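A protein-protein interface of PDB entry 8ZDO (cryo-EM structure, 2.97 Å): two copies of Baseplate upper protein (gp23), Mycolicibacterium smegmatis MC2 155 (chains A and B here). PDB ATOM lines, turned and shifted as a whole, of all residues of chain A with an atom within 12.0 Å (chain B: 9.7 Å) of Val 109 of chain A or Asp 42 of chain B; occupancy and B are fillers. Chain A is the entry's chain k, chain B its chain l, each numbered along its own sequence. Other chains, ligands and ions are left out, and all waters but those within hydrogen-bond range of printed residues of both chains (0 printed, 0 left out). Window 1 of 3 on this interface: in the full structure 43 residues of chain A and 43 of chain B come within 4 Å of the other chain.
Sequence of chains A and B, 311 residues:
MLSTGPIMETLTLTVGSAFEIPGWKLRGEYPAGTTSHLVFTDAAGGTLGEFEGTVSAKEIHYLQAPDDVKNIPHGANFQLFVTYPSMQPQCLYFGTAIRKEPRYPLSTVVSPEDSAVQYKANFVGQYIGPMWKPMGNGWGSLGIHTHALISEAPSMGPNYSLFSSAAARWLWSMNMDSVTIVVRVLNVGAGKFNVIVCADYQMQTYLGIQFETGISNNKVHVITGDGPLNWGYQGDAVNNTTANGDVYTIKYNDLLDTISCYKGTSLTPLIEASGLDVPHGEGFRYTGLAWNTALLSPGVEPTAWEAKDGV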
ATOM      1  N   VAL A  15     -24.329  13.862  -8.652  1.00  0.00           N
ATOM      2  CA  VAL A  15     -23.086  14.592  -8.433  1.00  0.00           C
ATOM      3  C   VAL A  15     -23.337  15.748  -7.474  1.00  0.00           C
ATOM      4  O   VAL A  15     -24.312  16.498  -7.615  1.00  0.00           O
ATOM      5  CB  VAL A  15     -22.493  15.078  -9.765  1.00  0.00           C
ATOM      6  CG1 VAL A  15     -22.049  13.898 -10.604  1.00  0.00           C
ATOM      7  CG2 VAL A  15     -23.507  15.910 -10.534  1.00  0.00           C
ATOM      8  N   GLU A 101     -29.256  12.662 -12.397  1.00  0.00           N
ATOM      9  CA  GLU A 101     -28.598  13.958 -12.358  1.00  0.00           C
ATOM     10  C   GLU A 101     -28.578  14.528 -13.766  1.00  0.00           C
ATOM     11  O   GLU A 101     -28.769  13.788 -14.738  1.00  0.00           O
ATOM     12  CB  GLU A 101     -27.169  13.833 -11.816  1.00  0.00           C
ATOM     13  CG  GLU A 101     -26.194  13.278 -12.831  1.00  0.00           C
ATOM     14  CD  GLU A 101     -24.916  12.802 -12.193  1.00  0.00           C
ATOM     15  OE1 GLU A 101     -24.901  12.648 -10.955  1.00  0.00           O
ATOM     16  OE2 GLU A 101     -23.930  12.577 -12.926  1.00  0.00           O
ATOM     17  N   PRO A 102     -28.368  15.835 -13.912  1.00  0.00           N
ATOM     18  CA  PRO A 102     -28.155  16.393 -15.250  1.00  0.00           C
ATOM     19  C   PRO A 102     -26.903  15.814 -15.895  1.00  0.00           C
ATOM     20  O   PRO A 102     -25.884  15.597 -15.237  1.00  0.00           O
ATOM     21  CB  PRO A 102     -28.013  17.897 -14.991  1.00  0.00           C
ATOM     22  CG  PRO A 102     -27.714  18.020 -13.538  1.00  0.00           C
ATOM     23  CD  PRO A 102     -28.422  16.885 -12.883  1.00  0.00           C
ATOM     24  N   ARG A 103     -26.991  15.568 -17.196  1.00  0.00           N
ATOM     25  CA  ARG A 103     -25.890  15.011 -17.966  1.00  0.00           C
ATOM     26  C   ARG A 103     -25.221  16.101 -18.790  1.00  0.00           C
ATOM     27  O   ARG A 103     -25.851  17.086 -19.182  1.00  0.00           O
ATOM     28  CB  ARG A 103     -26.376  13.890 -18.886  1.00  0.00           C
ATOM     29  CG  ARG A 103     -27.208  12.831 -18.192  1.00  0.00           C
ATOM     30  CD  ARG A 103     -26.355  11.989 -17.266  1.00  0.00           C
ATOM     31  NE  ARG A 103     -27.167  11.105 -16.440  1.00  0.00           N
ATOM     32  CZ  ARG A 103     -27.306   9.802 -16.648  1.00  0.00           C
ATOM     33  NH1 ARG A 103     -26.686   9.191 -17.643  1.00  0.00           N
ATOM     34  NH2 ARG A 103     -28.084   9.096 -15.833  1.00  0.00           N
ATOM     35  N   TYR A 104     -23.931  15.909 -19.057  1.00  0.00           N
ATOM     36  CA  TYR A 104     -23.131  16.852 -19.837  1.00  0.00           C
ATOM     37  C   TYR A 104     -22.452  16.101 -20.972  1.00  0.00           C
ATOM     38  O   TYR A 104     -21.239  15.861 -20.942  1.00  0.00           O
ATOM     39  CB  TYR A 104     -22.103  17.562 -18.957  1.00  0.00           C
ATOM     40  CG  TYR A 104     -22.686  18.168 -17.705  1.00  0.00           C
ATOM     41  CD1 TYR A 104     -23.719  19.089 -17.773  1.00  0.00           C
ATOM     42  CD2 TYR A 104     -22.201  17.820 -16.455  1.00  0.00           C
ATOM     43  CE1 TYR A 104     -24.253  19.645 -16.633  1.00  0.00           C
ATOM     44  CE2 TYR A 104     -22.730  18.371 -15.309  1.00  0.00           C
ATOM     45  CZ  TYR A 104     -23.756  19.282 -15.403  1.00  0.00           C
ATOM     46  OH  TYR A 104     -24.285  19.834 -14.260  1.00  0.00           O
ATOM     47  N   PRO A 105     -23.214  15.708 -21.995  1.00  0.00           N
ATOM     48  CA  PRO A 105     -22.607  14.970 -23.113  1.00  0.00           C
ATOM     49  C   PRO A 105     -21.593  15.785 -23.893  1.00  0.00           C
ATOM     50  O   PRO A 105     -20.670  15.208 -24.483  1.00  0.00           O
ATOM     51  CB  PRO A 105     -23.818  14.594 -23.973  1.00  0.00           C
ATOM     52  CG  PRO A 105     -24.823  15.654 -23.679  1.00  0.00           C
ATOM     53  CD  PRO A 105     -24.634  16.014 -22.235  1.00  0.00           C
ATOM     54  N   LEU A 106     -21.737  17.107 -23.922  1.00  0.00           N
ATOM     55  CA  LEU A 106     -20.785  17.947 -24.633  1.00  0.00           C
ATOM     56  C   LEU A 106     -19.492  18.065 -23.840  1.00  0.00           C
ATOM     57  O   LEU A 106     -19.514  18.268 -22.622  1.00  0.00           O
ATOM     58  CB  LEU A 106     -21.374  19.336 -24.883  1.00  0.00           C
ATOM     59  CG  LEU A 106     -22.379  19.510 -26.025  1.00  0.00           C
ATOM     60  CD1 LEU A 106     -23.728  18.901 -25.678  1.00  0.00           C
ATOM     61  CD2 LEU A 106     -22.530  20.979 -26.382  1.00  0.00           C
ATOM     62  N   SER A 107     -18.361  17.926 -24.532  1.00  0.00           N
ATOM     63  CA  SER A 107     -17.070  18.132 -23.885  1.00  0.00           C
ATOM     64  C   SER A 107     -16.895  19.587 -23.474  1.00  0.00           C
ATOM     65  O   SER A 107     -16.551  19.884 -22.324  1.00  0.00           O
ATOM     66  CB  SER A 107     -15.943  17.691 -24.817  1.00  0.00           C
ATOM     67  OG  SER A 107     -16.027  18.361 -26.062  1.00  0.00           O
ATOM     68  N   THR A 108     -17.133  20.510 -24.404  1.00  0.00           N
ATOM     69  CA  THR A 108     -17.114  21.938 -24.123  1.00  0.00           C
ATOM     70  C   THR A 108     -18.231  22.613 -24.901  1.00  0.00           C
ATOM     71  O   THR A 108     -18.629  22.152 -25.974  1.00  0.00           O
ATOM     72  CB  THR A 108     -15.775  22.593 -24.496  1.00  0.00           C
ATOM     73  OG1 THR A 108     -15.375  22.160 -25.803  1.00  0.00           O
ATOM     74  CG2 THR A 108     -14.693  22.240 -23.487  1.00  0.00           C
ATOM     75  N   VAL A 109     -18.735  23.709 -24.347  1.00  0.00           N
ATOM     76  CA  VAL A 109     -19.671  24.583 -25.041  1.00  0.00           C
ATOM     77  C   VAL A 109     -18.893  25.807 -25.496  1.00  0.00           C
ATOM     78  O   VAL A 109     -18.358  26.557 -24.671  1.00  0.00           O
ATOM     79  CB  VAL A 109     -20.858  24.974 -24.146  1.00  0.00           C
ATOM     80  CG1 VAL A 109     -21.531  26.228 -24.678  1.00  0.00           C
ATOM     81  CG2 VAL A 109     -21.859  23.836 -24.070  1.00  0.00           C
ATOM     82  N   VAL A 110     -18.814  26.000 -26.806  1.00  0.00           N
ATOM     83  CA  VAL A 110     -18.058  27.098 -27.389  1.00  0.00           C
ATOM     84  C   VAL A 110     -19.033  28.080 -28.017  1.00  0.00           C
ATOM     85  O   VAL A 110     -20.104  27.702 -28.509  1.00  0.00           O
ATOM     86  CB  VAL A 110     -17.031  26.600 -28.427  1.00  0.00           C
ATOM     87  CG1 VAL A 110     -15.967  25.756 -27.751  1.00  0.00           C
ATOM     88  CG2 VAL A 110     -17.723  25.805 -29.517  1.00  0.00           C
ATOM     89  N   SER A 111     -18.665  29.355 -27.982  1.00  0.00           N
ATOM     90  CA  SER A 111     -19.479  30.376 -28.618  1.00  0.00           C
ATOM     91  C   SER A 111     -19.523  30.118 -30.122  1.00  0.00           C
ATOM     92  O   SER A 111     -18.482  29.825 -30.724  1.00  0.00           O
ATOM     93  CB  SER A 111     -18.916  31.767 -28.332  1.00  0.00           C
ATOM     94  OG  SER A 111     -19.707  32.773 -28.939  1.00  0.00           O
ATOM     95  N   PRO A 112     -20.693  30.196 -30.753  1.00  0.00           N
ATOM     96  CA  PRO A 112     -20.772  29.905 -32.188  1.00  0.00           C
ATOM     97  C   PRO A 112     -19.951  30.891 -33.001  1.00  0.00           C
ATOM     98  O   PRO A 112     -19.807  32.062 -32.642  1.00  0.00           O
ATOM     99  CB  PRO A 112     -22.269  30.033 -32.496  1.00  0.00           C
ATOM    100  CG  PRO A 112     -22.811  30.900 -31.408  1.00  0.00           C
ATOM    101  CD  PRO A 112     -21.996  30.587 -30.189  1.00  0.00           C
ATOM    102  N   GLU A 113     -19.403  30.401 -34.111  1.00  0.00           N
ATOM    103  CA  GLU A 113     -18.594  31.243 -34.981  1.00  0.00           C
ATOM    104  C   GLU A 113     -19.492  32.202 -35.751  1.00  0.00           C
ATOM    105  O   GLU A 113     -19.901  31.919 -36.882  1.00  0.00           O
ATOM    106  CB  GLU A 113     -17.755  30.390 -35.937  1.00  0.00           C
ATOM    107  CG  GLU A 113     -16.898  31.190 -36.912  1.00  0.00           C
ATOM    108  CD  GLU A 113     -15.950  32.148 -36.216  1.00  0.00           C
ATOM    109  OE1 GLU A 113     -15.433  31.802 -35.132  1.00  0.00           O
ATOM    110  OE2 GLU A 113     -15.724  33.251 -36.754  1.00  0.00           O
ATOM    111  N   GLU A 282     -17.766  40.297 -25.904  1.00  0.00           N
ATOM    112  CA  GLU A 282     -19.193  40.001 -25.890  1.00  0.00           C
ATOM    113  C   GLU A 282     -19.929  40.953 -24.958  1.00  0.00           C
ATOM    114  O   GLU A 282     -19.438  41.300 -23.881  1.00  0.00           O
ATOM    115  CB  GLU A 282     -19.427  38.553 -25.458  1.00  0.00           C
ATOM    116  CG  GLU A 282     -19.449  37.556 -26.604  1.00  0.00           C
ATOM    117  CD  GLU A 282     -18.094  37.393 -27.265  1.00  0.00           C
ATOM    118  OE1 GLU A 282     -17.070  37.695 -26.615  1.00  0.00           O
ATOM    119  OE2 GLU A 282     -18.053  36.962 -28.436  1.00  0.00           O
ATOM    120  N   VAL B  39     -28.052  26.006  -8.575  1.00  0.00           N
ATOM    121  CA  VAL B  39     -26.934  26.070  -9.508  1.00  0.00           C
ATOM    122  C   VAL B  39     -27.460  25.839 -10.917  1.00  0.00           C
ATOM    123  O   VAL B  39     -28.174  24.862 -11.163  1.00  0.00           O
ATOM    124  CB  VAL B  39     -25.848  25.038  -9.157  1.00  0.00           C
ATOM    125  CG1 VAL B  39     -24.707  25.107 -10.154  1.00  0.00           C
ATOM    126  CG2 VAL B  39     -25.344  25.263  -7.744  1.00  0.00           C
ATOM    127  N   PHE B  40     -27.106  26.732 -11.835  1.00  0.00           N
ATOM    128  CA  PHE B  40     -27.460  26.625 -13.242  1.00  0.00           C
ATOM    129  C   PHE B  40     -26.197  26.383 -14.052  1.00  0.00           C
ATOM    130  O   PHE B  40     -25.251  27.176 -13.975  1.00  0.00           O
ATOM    131  CB  PHE B  40     -28.140  27.900 -13.744  1.00  0.00           C
ATOM    132  CG  PHE B  40     -29.523  28.103 -13.221  1.00  0.00           C
ATOM    133  CD1 PHE B  40     -29.730  28.761 -12.027  1.00  0.00           C
ATOM    134  CD2 PHE B  40     -30.618  27.661 -13.936  1.00  0.00           C
ATOM    135  CE1 PHE B  40     -31.001  28.960 -11.548  1.00  0.00           C
ATOM    136  CE2 PHE B  40     -31.892  27.859 -13.460  1.00  0.00           C
ATOM    137  CZ  PHE B  40     -32.082  28.511 -12.264  1.00  0.00           C
ATOM    138  N   THR B  41     -26.196  25.313 -14.843  1.00  0.00           N
ATOM    139  CA  THR B  41     -25.079  24.971 -15.708  1.00  0.00           C
ATOM    140  C   THR B  41     -25.575  24.811 -17.139  1.00  0.00           C
ATOM    141  O   THR B  41     -26.781  24.757 -17.407  1.00  0.00           O
ATOM    142  CB  THR B  41     -24.374  23.688 -15.246  1.00  0.00           C
ATOM    143  OG1 THR B  41     -25.254  22.570 -15.410  1.00  0.00           O
ATOM    144  CG2 THR B  41     -23.970  23.795 -13.785  1.00  0.00           C
ATOM    145  N   ASP B  42     -24.621  24.737 -18.060  1.00  0.00           N
ATOM    146  CA  ASP B  42     -24.883  24.589 -19.480  1.00  0.00           C
ATOM    147  C   ASP B  42     -24.675  23.136 -19.902  1.00  0.00           C
ATOM    148  O   ASP B  42     -24.509  22.237 -19.071  1.00  0.00           O
ATOM    149  CB  ASP B  42     -23.998  25.544 -20.281  1.00  0.00           C
ATOM    150  CG  ASP B  42     -22.524  25.371 -19.977  1.00  0.00           C
ATOM    151  OD1 ASP B  42     -22.183  24.515 -19.136  1.00  0.00           O
ATOM    152  OD2 ASP B  42     -21.704  26.095 -20.578  1.00  0.00           O
ATOM    153  N   ALA B  43     -24.690  22.899 -21.215  1.00  0.00           N
ATOM    154  CA  ALA B  43     -24.556  21.542 -21.733  1.00  0.00           C
ATOM    155  C   ALA B  43     -23.192  20.940 -21.421  1.00  0.00           C
ATOM    156  O   ALA B  43     -23.061  19.715 -21.337  1.00  0.00           O
ATOM    157  CB  ALA B  43     -24.805  21.533 -23.240  1.00  0.00           C
ATOM    158  N   ALA B  44     -22.168  21.773 -21.254  1.00  0.00           N
ATOM    159  CA  ALA B  44     -20.824  21.295 -20.960  1.00  0.00           C
ATOM    160  C   ALA B  44     -20.546  21.177 -19.469  1.00  0.00           C
ATOM    161  O   ALA B  44     -19.477  20.690 -19.091  1.00  0.00           O
ATOM    162  CB  ALA B  44     -19.783  22.216 -21.597  1.00  0.00           C
ATOM    163  N   GLY B  45     -21.476  21.602 -18.618  1.00  0.00           N
ATOM    164  CA  GLY B  45     -21.282  21.565 -17.188  1.00  0.00           C
ATOM    165  C   GLY B  45     -20.763  22.846 -16.578  1.00  0.00           C
ATOM    166  O   GLY B  45     -20.756  22.966 -15.347  1.00  0.00           O
ATOM    167  N   GLY B  46     -20.322  23.802 -17.392  1.00  0.00           N
ATOM    168  CA  GLY B  46     -19.866  25.077 -16.880  1.00  0.00           C
ATOM    169  C   GLY B  46     -20.954  25.824 -16.140  1.00  0.00           C
ATOM    170  O   GLY B  46     -22.050  26.024 -16.672  1.00  0.00           O
ATOM    171  N   THR B  47     -20.664  26.245 -14.913  1.00  0.00           N
ATOM    172  CA  THR B  47     -21.658  26.916 -14.082  1.00  0.00           C
ATOM    173  C   THR B  47     -21.932  28.304 -14.642  1.00  0.00           C
ATOM    174  O   THR B  47     -21.058  29.177 -14.616  1.00  0.00           O
ATOM    175  CB  THR B  47     -21.173  26.998 -12.639  1.00  0.00           C
ATOM    176  OG1 THR B  47     -21.180  25.689 -12.057  1.00  0.00           O
ATOM    177  CG2 THR B  47     -22.079  27.907 -11.825  1.00  0.00           C
ATOM    178  N   LEU B  48     -23.140  28.508 -15.159  1.00  0.00           N
ATOM    179  CA  LEU B  48     -23.556  29.810 -15.654  1.00  0.00           C
ATOM    180  C   LEU B  48     -24.401  30.579 -14.650  1.00  0.00           C
ATOM    181  O   LEU B  48     -24.848  31.687 -14.958  1.00  0.00           O
ATOM    182  CB  LEU B  48     -24.314  29.655 -16.978  1.00  0.00           C
ATOM    183  CG  LEU B  48     -25.532  28.735 -17.038  1.00  0.00           C
ATOM    184  CD1 LEU B  48     -26.804  29.483 -16.704  1.00  0.00           C
ATOM    185  CD2 LEU B  48     -25.638  28.107 -18.409  1.00  0.00           C
ATOM    186  N   GLY B  49     -24.638  30.021 -13.466  1.00  0.00           N
ATOM    187  CA  GLY B  49     -25.322  30.775 -12.434  1.00  0.00           C
ATOM    188  C   GLY B  49     -25.358  30.091 -11.084  1.00  0.00           C
ATOM    189  O   GLY B  49     -25.379  28.861 -11.009  1.00  0.00           O
ATOM    190  N   ASN B  71     -29.065  35.938 -18.318  1.00  0.00           N
ATOM    191  CA  ASN B  71     -28.017  35.221 -19.034  1.00  0.00           C
ATOM    192  C   ASN B  71     -28.214  33.712 -19.029  1.00  0.00           C
ATOM    193  O   ASN B  71     -27.396  32.996 -19.614  1.00  0.00           O
ATOM    194  CB  ASN B  71     -26.648  35.560 -18.439  1.00  0.00           C
ATOM    195  CG  ASN B  71     -26.639  35.498 -16.925  1.00  0.00           C
ATOM    196  OD1 ASN B  71     -27.663  35.234 -16.299  1.00  0.00           O
ATOM    197  ND2 ASN B  71     -25.478  35.740 -16.329  1.00  0.00           N
ATOM    198  N   ILE B  72     -29.268  33.210 -18.391  1.00  0.00           N
ATOM    199  CA  ILE B  72     -29.535  31.776 -18.320  1.00  0.00           C
ATOM    200  C   ILE B  72     -30.399  31.404 -19.522  1.00  0.00           C
ATOM    201  O   ILE B  72     -31.545  31.874 -19.611  1.00  0.00           O
ATOM    202  CB  ILE B  72     -30.225  31.397 -17.005  1.00  0.00           C
ATOM    203  CG1 ILE B  72     -29.368  31.817 -15.812  1.00  0.00           C
ATOM    204  CG2 ILE B  72     -30.494  29.905 -16.960  1.00  0.00           C
ATOM    205  CD1 ILE B  72     -30.082  31.720 -14.491  1.00  0.00           C
ATOM    206  N   PRO B  73     -29.909  30.586 -20.447  1.00  0.00           N
ATOM    207  CA  PRO B  73     -30.700  30.239 -21.628  1.00  0.00           C
ATOM    208  C   PRO B  73     -31.705  29.136 -21.335  1.00  0.00           C
ATOM    209  O   PRO B  73     -31.620  28.425 -20.334  1.00  0.00           O
ATOM    210  CB  PRO B  73     -29.640  29.761 -22.624  1.00  0.00           C
ATOM    211  CG  PRO B  73     -28.584  29.166 -21.757  1.00  0.00           C
ATOM    212  CD  PRO B  73     -28.585  29.941 -20.460  1.00  0.00           C
ATOM    213  N   HIS B  74     -32.677  29.009 -22.234  1.00  0.00           N
ATOM    214  CA  HIS B  74     -33.600  27.888 -22.154  1.00  0.00           C
ATOM    215  C   HIS B  74     -32.857  26.604 -22.495  1.00  0.00           C
ATOM    216  O   HIS B  74     -32.058  26.560 -23.433  1.00  0.00           O
ATOM    217  CB  HIS B  74     -34.783  28.083 -23.101  1.00  0.00           C
ATOM    218  CG  HIS B  74     -34.405  28.088 -24.548  1.00  0.00           C
ATOM    219  ND1 HIS B  74     -33.886  29.196 -25.179  1.00  0.00           N
ATOM    220  CD2 HIS B  74     -34.475  27.116 -25.489  1.00  0.00           C
ATOM    221  CE1 HIS B  74     -33.649  28.908 -26.447  1.00  0.00           C
ATOM    222  NE2 HIS B  74     -33.997  27.652 -26.660  1.00  0.00           N
ATOM    223  N   GLY B  75     -33.120  25.557 -21.724  1.00  0.00           N
ATOM    224  CA  GLY B  75     -32.361  24.335 -21.827  1.00  0.00           C
ATOM    225  C   GLY B  75     -31.192  24.239 -20.875  1.00  0.00           C
ATOM    226  O   GLY B  75     -30.627  23.149 -20.723  1.00  0.00           O
ATOM    227  N   ALA B  76     -30.806  25.339 -20.234  1.00  0.00           N
ATOM    228  CA  ALA B  76     -29.809  25.270 -19.178  1.00  0.00           C
ATOM    229  C   ALA B  76     -30.358  24.456 -18.018  1.00  0.00           C
ATOM    230  O   ALA B  76     -31.529  24.580 -17.652  1.00  0.00           O
ATOM    231  CB  ALA B  76     -29.423  26.670 -18.707  1.00  0.00           C
ATOM    232  N   ASN B  77     -29.512  23.616 -17.438  1.00  0.00           N
ATOM    233  CA  ASN B  77     -29.969  22.649 -16.450  1.00  0.00           C
ATOM    234  C   ASN B  77     -29.628  23.117 -15.042  1.00  0.00           C
ATOM    235  O   ASN B  77     -28.513  23.575 -14.780  1.00  0.00           O
ATOM    236  CB  ASN B  77     -29.402  21.257 -16.751  1.00  0.00           C
ATOM    237  CG  ASN B  77     -27.890  21.232 -16.852  1.00  0.00           C
ATOM    238  OD1 ASN B  77     -27.213  22.215 -16.576  1.00  0.00           O
ATOM    239  ND2 ASN B  77     -27.357  20.102 -17.289  1.00  0.00           N
ATOM    240  N   PHE B  78     -30.606  23.028 -14.149  1.00  0.00           N
ATOM    241  CA  PHE B  78     -30.478  23.531 -12.793  1.00  0.00           C
ATOM    242  C   PHE B  78     -30.400  22.380 -11.801  1.00  0.00           C
ATOM    243  O   PHE B  78     -30.664  21.219 -12.120  1.00  0.00           O
ATOM    244  CB  PHE B  78     -31.640  24.466 -12.444  1.00  0.00           C
ATOM    245  CG  PHE B  78     -32.927  23.757 -12.134  1.00  0.00           C
ATOM    246  CD1 PHE B  78     -33.785  23.378 -13.150  1.00  0.00           C
ATOM    247  CD2 PHE B  78     -33.289  23.489 -10.827  1.00  0.00           C
ATOM    248  CE1 PHE B  78     -34.969  22.733 -12.870  1.00  0.00           C
ATOM    249  CE2 PHE B  78     -34.471  22.843 -10.541  1.00  0.00           C
ATOM    250  CZ  PHE B  78     -35.313  22.466 -11.563  1.00  0.00           C
ATOM    251  N   GLN B  79     -30.019  22.733 -10.579  1.00  0.00           N
ATOM    252  CA  GLN B  79     -29.854  21.763  -9.504  1.00  0.00           C
ATOM    253  C   GLN B  79     -30.001  22.509  -8.191  1.00  0.00           C
ATOM    254  O   GLN B  79     -29.235  23.438  -7.922  1.00  0.00           O
ATOM    255  CB  GLN B  79     -28.494  21.084  -9.601  1.00  0.00           C
ATOM    256  CG  GLN B  79     -28.471  19.650  -9.132  1.00  0.00           C
ATOM    257  CD  GLN B  79     -27.202  18.940  -9.544  1.00  0.00           C
ATOM    258  OE1 GLN B  79     -26.333  19.526 -10.186  1.00  0.00           O
ATOM    259  NE2 GLN B  79     -27.087  17.672  -9.178  1.00  0.00           N
ATOM    260  N   GLY B  95     -33.333  19.548 -13.061  1.00  0.00           N
ATOM    261  CA  GLY B  95     -34.099  19.559 -14.288  1.00  0.00           C
ATOM    262  C   GLY B  95     -33.645  20.585 -15.298  1.00  0.00           C
ATOM    263  O   GLY B  95     -32.445  20.787 -15.499  1.00  0.00           O
ATOM    264  N   THR B  96     -34.604  21.241 -15.944  1.00  0.00           N
ATOM    265  CA  THR B  96     -34.328  22.179 -17.017  1.00  0.00           C
ATOM    266  C   THR B  96     -35.086  23.475 -16.768  1.00  0.00           C
ATOM    267  O   THR B  96     -36.187  23.478 -16.208  1.00  0.00           O
ATOM    268  CB  THR B  96     -34.710  21.575 -18.380  1.00  0.00           C
ATOM    269  OG1 THR B  96     -33.955  20.377 -18.596  1.00  0.00           O
ATOM    270  CG2 THR B  96     -34.420  22.540 -19.513  1.00  0.00           C
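O of Val 15 of chain A sits at hydrogen-bond distance from NE2 of Gln 79 of chain B (3.4 Å). The side-chain hydroxyl (OH) of Tyr 104 of chain A is in hydrogen-bond range of the side-chain hydroxyl (OG1) of Thr 41 of chain B, at 3.1 Å.
Hydrophobic or aromatic side chains of chain B that line the printed part of chain A: Ala 43 and Ala 44. Among the printed residues, 16 pairs touch across the chains. Among the printed residues, no Asp or Glu carboxylate lies within 4 Å of a Lys or Arg side-chain nitrogen of the other chain.
The backbone NH of Gly 45 of chain B sits at hydrogen-bond distance from the side-chain carboxylate of Asp 42 of chain B (3.0 Å). The side-chain carboxylate (OD1) of Asp 42 of chain B is in hydrogen-bond range of the backbone NH (N) of Gly 46 of chain B (2.6 Å). N of Ala 44 of chain B sits close to OD1 of Asp 42 of chain B. The side-chain carboxylate of Glu 101 of chain A lies within hydrogen-bond range of the backbone NH of Val 15 of chain A (2.7 Å). O of Val 39 of chain B sits at hydrogen-bond distance from N of Gln 79 of chain B. The backbone carbonyl oxygen (O) of Thr 41 of chain B sits close to the side-chain amide oxygen (OD1) of Asn 77 of chain B (2.7 Å).
CB of Pro 102 of chain A touches ND2 of Asn 77 of chain B, at 3.3 Å. Gln 79 of chain B touches Pro 102 of chain A. Asn 77 of chain B touches Arg 103 of chain A. Tyr 104 of chain A touches Asp 42 of chain B. Tyr 104 of chain A touches Ala 43 of chain B. C of Ala 44 of chain B touches CB of Tyr 104 of chain A, 3.97 Å away. Ala 44 of chain B touches Leu 106 of chain A (CA to O, 3.7 Å). Ala 44 of chain B touches Thr 108 of chain A (CB to C, 3.7 Å). Val 109 of chain A touches Ala 43 of chain B. Val 109 of chain A touches Ala 44 of chain B.
No position is printed for both chains. Of the 16 pairs that touch across the chains among the printed residues, none has its exchanged pair printed and touching as well.
Of chain B, only Asp 42 (3.8 Å), Ala 43 (3.8 Å) and Ala 44 (3.3 Å) come within 4 Å of Val 109 of chain A. Of chain A, only Tyr 104 and Val 109 come within 4 Å of Asp 42 of chain B. Thr 108 of chain A touches just one residue of chain B: Ala 44. Ala 43 of chain B touches three residues of chain A. Ala 44 of chain B touches four residues of chain A. Gly 45 of chain B touches just one residue of chain A: Tyr 104 (3.5 Å). No residue of chain A comes within 4 Å of Thr 47 of chain B. No residue of chain A comes within 4 Å of Leu 48 of chain B. Ala 76 of chain B touches none of the printed residues of chain A. Of the printed residues of chain B, Arg 103 of chain A touches Asn 77 (3.9 Å). Printed residues of chain B within 4 Å of Leu 106 of chain A: Ala 43 (3.7 Å) and Ala 44 (3.7 Å). The nearest residue of chain B that does not touch Val 109 of chain A is Gly 45 of chain B (5.9 Å). The nearest printed residue of chain B that does not touch Leu 106 of chain A is Gly 45 of chain B (5.6 Å).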
